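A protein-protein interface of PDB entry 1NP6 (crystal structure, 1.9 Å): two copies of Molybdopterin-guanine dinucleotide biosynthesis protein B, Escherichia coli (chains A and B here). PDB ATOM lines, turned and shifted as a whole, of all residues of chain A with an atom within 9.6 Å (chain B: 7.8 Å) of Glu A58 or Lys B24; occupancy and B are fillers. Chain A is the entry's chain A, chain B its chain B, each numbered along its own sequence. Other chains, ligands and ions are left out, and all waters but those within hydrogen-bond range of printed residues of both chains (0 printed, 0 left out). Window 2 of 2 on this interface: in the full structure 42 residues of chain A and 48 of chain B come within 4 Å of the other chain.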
ATOM      1  N   GLU A  58       5.057  21.371   0.107  1.00  0.00           N
ATOM      2  CA  GLU A  58       4.415  22.336  -0.781  1.00  0.00           C
ATOM      3  C   GLU A  58       4.980  23.759  -0.671  1.00  0.00           C
ATOM      4  O   GLU A  58       5.058  24.464  -1.678  1.00  0.00           O
ATOM      5  CB  GLU A  58       2.899  22.348  -0.561  1.00  0.00           C
ATOM      6  CG  GLU A  58       2.100  22.337  -1.854  1.00  0.00           C
ATOM      7  CD  GLU A  58       0.845  21.484  -1.772  1.00  0.00           C
ATOM      8  OE1 GLU A  58      -0.265  22.031  -1.966  1.00  0.00           O
ATOM      9  OE2 GLU A  58       0.969  20.265  -1.523  1.00  0.00           O
ATOM     10  N   LEU A  59       5.361  24.171   0.541  1.00  0.00           N
ATOM     11  CA  LEU A  59       5.930  25.505   0.792  1.00  0.00           C
ATOM     12  C   LEU A  59       7.430  25.577   0.475  1.00  0.00           C
ATOM     13  O   LEU A  59       7.995  26.668   0.315  1.00  0.00           O
ATOM     14  CB  LEU A  59       5.686  25.943   2.239  1.00  0.00           C
ATOM     15  CG  LEU A  59       4.242  26.061   2.721  1.00  0.00           C
ATOM     16  CD1 LEU A  59       4.034  25.188   3.947  1.00  0.00           C
ATOM     17  CD2 LEU A  59       3.901  27.504   3.023  1.00  0.00           C
ATOM     18  N   ARG A  60       8.069  24.411   0.412  1.00  0.00           N
ATOM     19  CA  ARG A  60       9.433  24.300  -0.095  1.00  0.00           C
ATOM     20  C   ARG A  60       9.386  24.403  -1.618  1.00  0.00           C
ATOM     21  O   ARG A  60      10.226  25.067  -2.231  1.00  0.00           O
ATOM     22  CB  ARG A  60      10.066  22.973   0.332  1.00  0.00           C
ATOM     23  CG  ARG A  60      10.359  22.859   1.824  1.00  0.00           C
ATOM     24  CD  ARG A  60      11.667  22.153   2.146  1.00  0.00           C
ATOM     25  NE  ARG A  60      11.517  20.697   2.172  1.00  0.00           N
ATOM     26  CZ  ARG A  60      11.912  19.875   1.202  1.00  0.00           C
ATOM     27  NH1 ARG A  60      12.489  20.346   0.099  1.00  0.00           N
ATOM     28  NH2 ARG A  60      11.728  18.569   1.337  1.00  0.00           N
ATOM     29  N   LYS A  61       8.390  23.742  -2.211  1.00  0.00           N
ATOM     30  CA  LYS A  61       8.091  23.830  -3.642  1.00  0.00           C
ATOM     31  C   LYS A  61       7.664  25.251  -4.038  1.00  0.00           C
ATOM     32  O   LYS A  61       7.887  25.684  -5.176  1.00  0.00           O
ATOM     33  CB  LYS A  61       6.983  22.835  -4.001  1.00  0.00           C
ATOM     34  CG  LYS A  61       7.210  22.075  -5.294  1.00  0.00           C
ATOM     35  CD  LYS A  61       5.990  22.158  -6.197  1.00  0.00           C
ATOM     36  CE  LYS A  61       6.248  21.485  -7.536  1.00  0.00           C
ATOM     37  NZ  LYS A  61       5.250  20.408  -7.800  1.00  0.00           N
ATOM     38  N   ALA A  62       7.042  25.957  -3.091  1.00  0.00           N
ATOM     39  CA  ALA A  62       6.633  27.349  -3.269  1.00  0.00           C
ATOM     40  C   ALA A  62       7.854  28.268  -3.279  1.00  0.00           C
ATOM     41  O   ALA A  62       7.847  29.322  -3.921  1.00  0.00           O
ATOM     42  CB  ALA A  62       5.649  27.759  -2.178  1.00  0.00           C
ATOM     43  N   GLY A  63       8.897  27.868  -2.553  1.00  0.00           N
ATOM     44  CA  GLY A  63      10.200  28.470  -2.740  1.00  0.00           C
ATOM     45  C   GLY A  63      10.951  28.996  -1.532  1.00  0.00           C
ATOM     46  O   GLY A  63      11.760  29.902  -1.697  1.00  0.00           O
ATOM     47  N   ALA A  64      10.727  28.456  -0.336  1.00  0.00           N
ATOM     48  CA  ALA A  64      11.639  28.806   0.759  1.00  0.00           C
ATOM     49  C   ALA A  64      12.914  27.980   0.645  1.00  0.00           C
ATOM     50  O   ALA A  64      12.881  26.751   0.725  1.00  0.00           O
ATOM     51  CB  ALA A  64      10.979  28.666   2.150  1.00  0.00           C
ATOM     52  N   THR A  67      14.179  26.070   5.483  1.00  0.00           N
ATOM     53  CA  THR A  67      12.969  25.802   6.274  1.00  0.00           C
ATOM     54  C   THR A  67      13.319  25.076   7.577  1.00  0.00           C
ATOM     55  O   THR A  67      14.017  24.064   7.544  1.00  0.00           O
ATOM     56  CB  THR A  67      11.944  24.953   5.416  1.00  0.00           C
ATOM     57  OG1 THR A  67      11.481  25.740   4.321  1.00  0.00           O
ATOM     58  CG2 THR A  67      10.633  24.698   6.169  1.00  0.00           C
ATOM     59  N   GLY B  18      -6.795  30.343   7.266  1.00  0.00           N
ATOM     60  CA  GLY B  18      -6.139  30.262   5.967  1.00  0.00           C
ATOM     61  C   GLY B  18      -4.661  30.633   5.935  1.00  0.00           C
ATOM     62  O   GLY B  18      -4.137  30.985   4.887  1.00  0.00           O
ATOM     63  N   LYS B  19      -3.996  30.563   7.084  1.00  0.00           N
ATOM     64  CA  LYS B  19      -2.558  30.822   7.210  1.00  0.00           C
ATOM     65  C   LYS B  19      -1.620  30.087   6.213  1.00  0.00           C
ATOM     66  O   LYS B  19      -0.885  30.742   5.459  1.00  0.00           O
ATOM     67  CB  LYS B  19      -2.128  30.502   8.636  1.00  0.00           C
ATOM     68  CG  LYS B  19      -1.458  31.632   9.325  1.00  0.00           C
ATOM     69  CD  LYS B  19      -0.600  31.129  10.458  1.00  0.00           C
ATOM     70  CE  LYS B  19      -1.412  30.927  11.714  1.00  0.00           C
ATOM     71  NZ  LYS B  19      -1.478  29.484  12.105  1.00  0.00           N
ATOM     72  N   THR B  20      -1.609  28.751   6.229  1.00  0.00           N
ATOM     73  CA  THR B  20      -0.641  28.003   5.394  1.00  0.00           C
ATOM     74  C   THR B  20      -0.905  28.189   3.886  1.00  0.00           C
ATOM     75  O   THR B  20       0.034  28.324   3.081  1.00  0.00           O
ATOM     76  CB  THR B  20      -0.529  26.487   5.772  1.00  0.00           C
ATOM     77  OG1 THR B  20      -1.529  25.727   5.081  1.00  0.00           O
ATOM     78  CG2 THR B  20      -0.803  26.232   7.261  1.00  0.00           C
ATOM     79  N   THR B  21      -2.186  28.229   3.533  1.00  0.00           N
ATOM     80  CA  THR B  21      -2.642  28.501   2.170  1.00  0.00           C
ATOM     81  C   THR B  21      -2.179  29.873   1.656  1.00  0.00           C
ATOM     82  O   THR B  21      -1.775  30.011   0.499  1.00  0.00           O
ATOM     83  CB  THR B  21      -4.187  28.386   2.123  1.00  0.00           C
ATOM     84  OG1 THR B  21      -4.553  27.003   2.062  1.00  0.00           O
ATOM     85  CG2 THR B  21      -4.788  28.997   0.854  1.00  0.00           C
ATOM     86  N   LEU B  22      -2.256  30.881   2.524  1.00  0.00           N
ATOM     87  CA  LEU B  22      -1.802  32.225   2.212  1.00  0.00           C
ATOM     88  C   LEU B  22      -0.294  32.239   1.992  1.00  0.00           C
ATOM     89  O   LEU B  22       0.175  32.800   1.009  1.00  0.00           O
ATOM     90  CB  LEU B  22      -2.202  33.217   3.327  1.00  0.00           C
ATOM     91  CG  LEU B  22      -1.817  34.686   3.054  1.00  0.00           C
ATOM     92  CD1 LEU B  22      -2.412  35.203   1.745  1.00  0.00           C
ATOM     93  CD2 LEU B  22      -2.216  35.596   4.193  1.00  0.00           C
ATOM     94  N   LEU B  23       0.456  31.641   2.924  1.00  0.00           N
ATOM     95  CA  LEU B  23       1.920  31.553   2.834  1.00  0.00           C
ATOM     96  C   LEU B  23       2.379  30.807   1.572  1.00  0.00           C
ATOM     97  O   LEU B  23       3.408  31.151   0.982  1.00  0.00           O
ATOM     98  CB  LEU B  23       2.504  30.916   4.083  1.00  0.00           C
ATOM     99  CG  LEU B  23       3.104  31.772   5.200  1.00  0.00           C
ATOM    100  CD1 LEU B  23       2.769  33.255   5.123  1.00  0.00           C
ATOM    101  CD2 LEU B  23       2.763  31.185   6.579  1.00  0.00           C
ATOM    102  N   LYS B  24       1.592  29.814   1.155  1.00  0.00           N
ATOM    103  CA  LYS B  24       1.832  29.047  -0.077  1.00  0.00           C
ATOM    104  C   LYS B  24       1.900  29.905  -1.328  1.00  0.00           C
ATOM    105  O   LYS B  24       2.639  29.569  -2.250  1.00  0.00           O
ATOM    106  CB  LYS B  24       0.757  27.967  -0.273  1.00  0.00           C
ATOM    107  CG  LYS B  24       1.069  26.658   0.403  1.00  0.00           C
ATOM    108  CD  LYS B  24       0.481  25.489  -0.372  1.00  0.00           C
ATOM    109  CE  LYS B  24      -0.251  24.517   0.543  1.00  0.00           C
ATOM    110  NZ  LYS B  24      -1.510  24.021  -0.086  1.00  0.00           N
ATOM    111  N   LYS B  25       1.136  31.003  -1.358  1.00  0.00           N
ATOM    112  CA  LYS B  25       1.147  31.966  -2.472  1.00  0.00           C
ATOM    113  C   LYS B  25       2.020  33.215  -2.252  1.00  0.00           C
ATOM    114  O   LYS B  25       2.460  33.847  -3.210  1.00  0.00           O
ATOM    115  CB  LYS B  25      -0.272  32.444  -2.818  1.00  0.00           C
ATOM    116  CG  LYS B  25      -1.400  31.479  -2.489  1.00  0.00           C
ATOM    117  CD  LYS B  25      -2.625  31.771  -3.333  1.00  0.00           C
ATOM    118  CE  LYS B  25      -3.517  32.817  -2.684  1.00  0.00           C
ATOM    119  NZ  LYS B  25      -4.330  33.576  -3.684  1.00  0.00           N
ATOM    120  N   LEU B  26       2.244  33.602  -1.001  1.00  0.00           N
ATOM    121  CA  LEU B  26       3.040  34.802  -0.733  1.00  0.00           C
ATOM    122  C   LEU B  26       4.526  34.580  -0.980  1.00  0.00           C
ATOM    123  O   LEU B  26       5.205  35.460  -1.543  1.00  0.00           O
ATOM    124  CB  LEU B  26       2.802  35.288   0.715  1.00  0.00           C
ATOM    125  CG  LEU B  26       3.651  36.484   1.163  1.00  0.00           C
ATOM    126  CD1 LEU B  26       3.299  37.765   0.403  1.00  0.00           C
ATOM    127  CD2 LEU B  26       3.529  36.669   2.699  1.00  0.00           C
ATOM    128  N   ILE B  27       5.029  33.410  -0.570  1.00  0.00           N
ATOM    129  CA  ILE B  27       6.446  33.067  -0.691  1.00  0.00           C
ATOM    130  C   ILE B  27       6.940  33.119  -2.163  1.00  0.00           C
ATOM    131  O   ILE B  27       7.953  33.758  -2.452  1.00  0.00           O
ATOM    132  CB  ILE B  27       6.761  31.716   0.023  1.00  0.00           C
ATOM    133  CG1 ILE B  27       6.756  31.910   1.559  1.00  0.00           C
ATOM    134  CG2 ILE B  27       8.120  31.144  -0.410  1.00  0.00           C
ATOM    135  CD1 ILE B  27       6.624  30.602   2.369  1.00  0.00           C
ATOM    136  N   PRO B  28       6.232  32.480  -3.089  1.00  0.00           N
ATOM    137  CA  PRO B  28       6.579  32.621  -4.519  1.00  0.00           C
ATOM    138  C   PRO B  28       6.611  34.073  -4.981  1.00  0.00           C
ATOM    139  O   PRO B  28       7.548  34.449  -5.690  1.00  0.00           O
ATOM    140  CB  PRO B  28       5.456  31.846  -5.246  1.00  0.00           C
ATOM    141  CG  PRO B  28       4.956  30.855  -4.245  1.00  0.00           C
ATOM    142  CD  PRO B  28       5.107  31.542  -2.877  1.00  0.00           C
ATOM    143  N   ALA B  29       5.604  34.862  -4.575  1.00  0.00           N
ATOM    144  CA  ALA B  29       5.492  36.257  -4.925  1.00  0.00           C
ATOM    145  C   ALA B  29       6.668  37.078  -4.397  1.00  0.00           C
ATOM    146  O   ALA B  29       7.179  37.966  -5.086  1.00  0.00           O
ATOM    147  CB  ALA B  29       4.184  36.817  -4.424  1.00  0.00           C
ATOM    148  N   GLU B 107       5.468  30.863  11.617  1.00  0.00           N
ATOM    149  CA  GLU B 107       4.088  30.357  11.634  1.00  0.00           C
ATOM    150  C   GLU B 107       3.823  29.119  12.536  1.00  0.00           C
ATOM    151  O   GLU B 107       4.647  28.209  12.622  1.00  0.00           O
ATOM    152  CB  GLU B 107       3.691  30.020  10.189  1.00  0.00           C
ATOM    153  CG  GLU B 107       2.500  29.101  10.067  1.00  0.00           C
ATOM    154  CD  GLU B 107       2.488  28.366   8.755  1.00  0.00           C
ATOM    155  OE1 GLU B 107       3.523  27.763   8.402  1.00  0.00           O
ATOM    156  OE2 GLU B 107       1.443  28.410   8.077  1.00  0.00           O
ATOM    157  N   VAL B 158      -2.727  39.249  -2.972  1.00  0.00           N
ATOM    158  CA  VAL B 158      -1.389  38.715  -2.697  1.00  0.00           C
ATOM    159  C   VAL B 158      -0.221  39.618  -3.132  1.00  0.00           C
ATOM    160  O   VAL B 158       0.756  39.779  -2.375  1.00  0.00           O
ATOM    161  CB  VAL B 158      -1.214  37.278  -3.271  1.00  0.00           C
ATOM    162  CG1 VAL B 158       0.183  36.726  -2.981  1.00  0.00           C
ATOM    163  CG2 VAL B 158      -2.277  36.339  -2.713  1.00  0.00           C
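Printed residues of chain B that touch a printed residue of chain A: Thr B20, Leu B23, Lys B24, Ile B27 and Pro B28. Hydrophobic or aromatic side chains of chain B within 4 Å of the printed part of chain A: Leu B23, Ile B27 and Pro B28. Of the 8 printed residues of chain A, 5 touch a printed residue of chain B. Hydrophobic or aromatic side chains of chain A that line the printed part of chain B: Leu A59 and Ala A62. Among the printed residues, 9 pairs touch across the chains. Among the printed residues, Asp or Glu carboxylates within 4 Å of a Lys or Arg side-chain nitrogen of the other chain: Glu A58 with Lys B24.
No position is printed for both chains.
Glu A58 touches one residue of chain B. Printed residues of chain B within 4 Å of Ala A62: Lys B24 (3.5 Å), Ile B27 (3.97 Å) and Pro B28 (3.3 Å). Of the printed residues of chain B, Gly A63 touches Ile B27. Of the printed residues of chain B, Ala A64 touches Ile B27. Printed residues of chain A within 4 Å of Thr B20: Leu A59 (3.95 Å). Lys B24 touches just these residues of chain A: Glu A58, Leu A59 and Ala A62. Lys B25 touches none of the printed residues of chain A. The nearest residue of chain B that does not touch Glu A58 is Pro B28 (6.9 Å).
CD2 of Leu A59 touches O of Thr B20, at 3.95 Å. CB of Leu B23 touches CD2 of Leu A59, 3.8 Å away. Leu A59 touches Lys B24 (CD2 to N, 3.8 Å). Lys B24 touches Ala A62. Ala A62 touches Ile B27 (O to CG2, 3.97 Å). CG of Pro B28 touches O of Ala A62, 3.3 Å away. Gly A63 touches Ile B27 (C to CG2, 3.7 Å). Ile B27 touches Ala A64 (CG2 to N, 3.7 Å).
OE1 of Glu A58 lies within salt-bridge range of NZ of Lys B24, at 3.0 Å.
The backbone carbonyl oxygen of Leu A59 is in hydrogen-bond range of the backbone NH of Ala A64 (3.3 Å).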
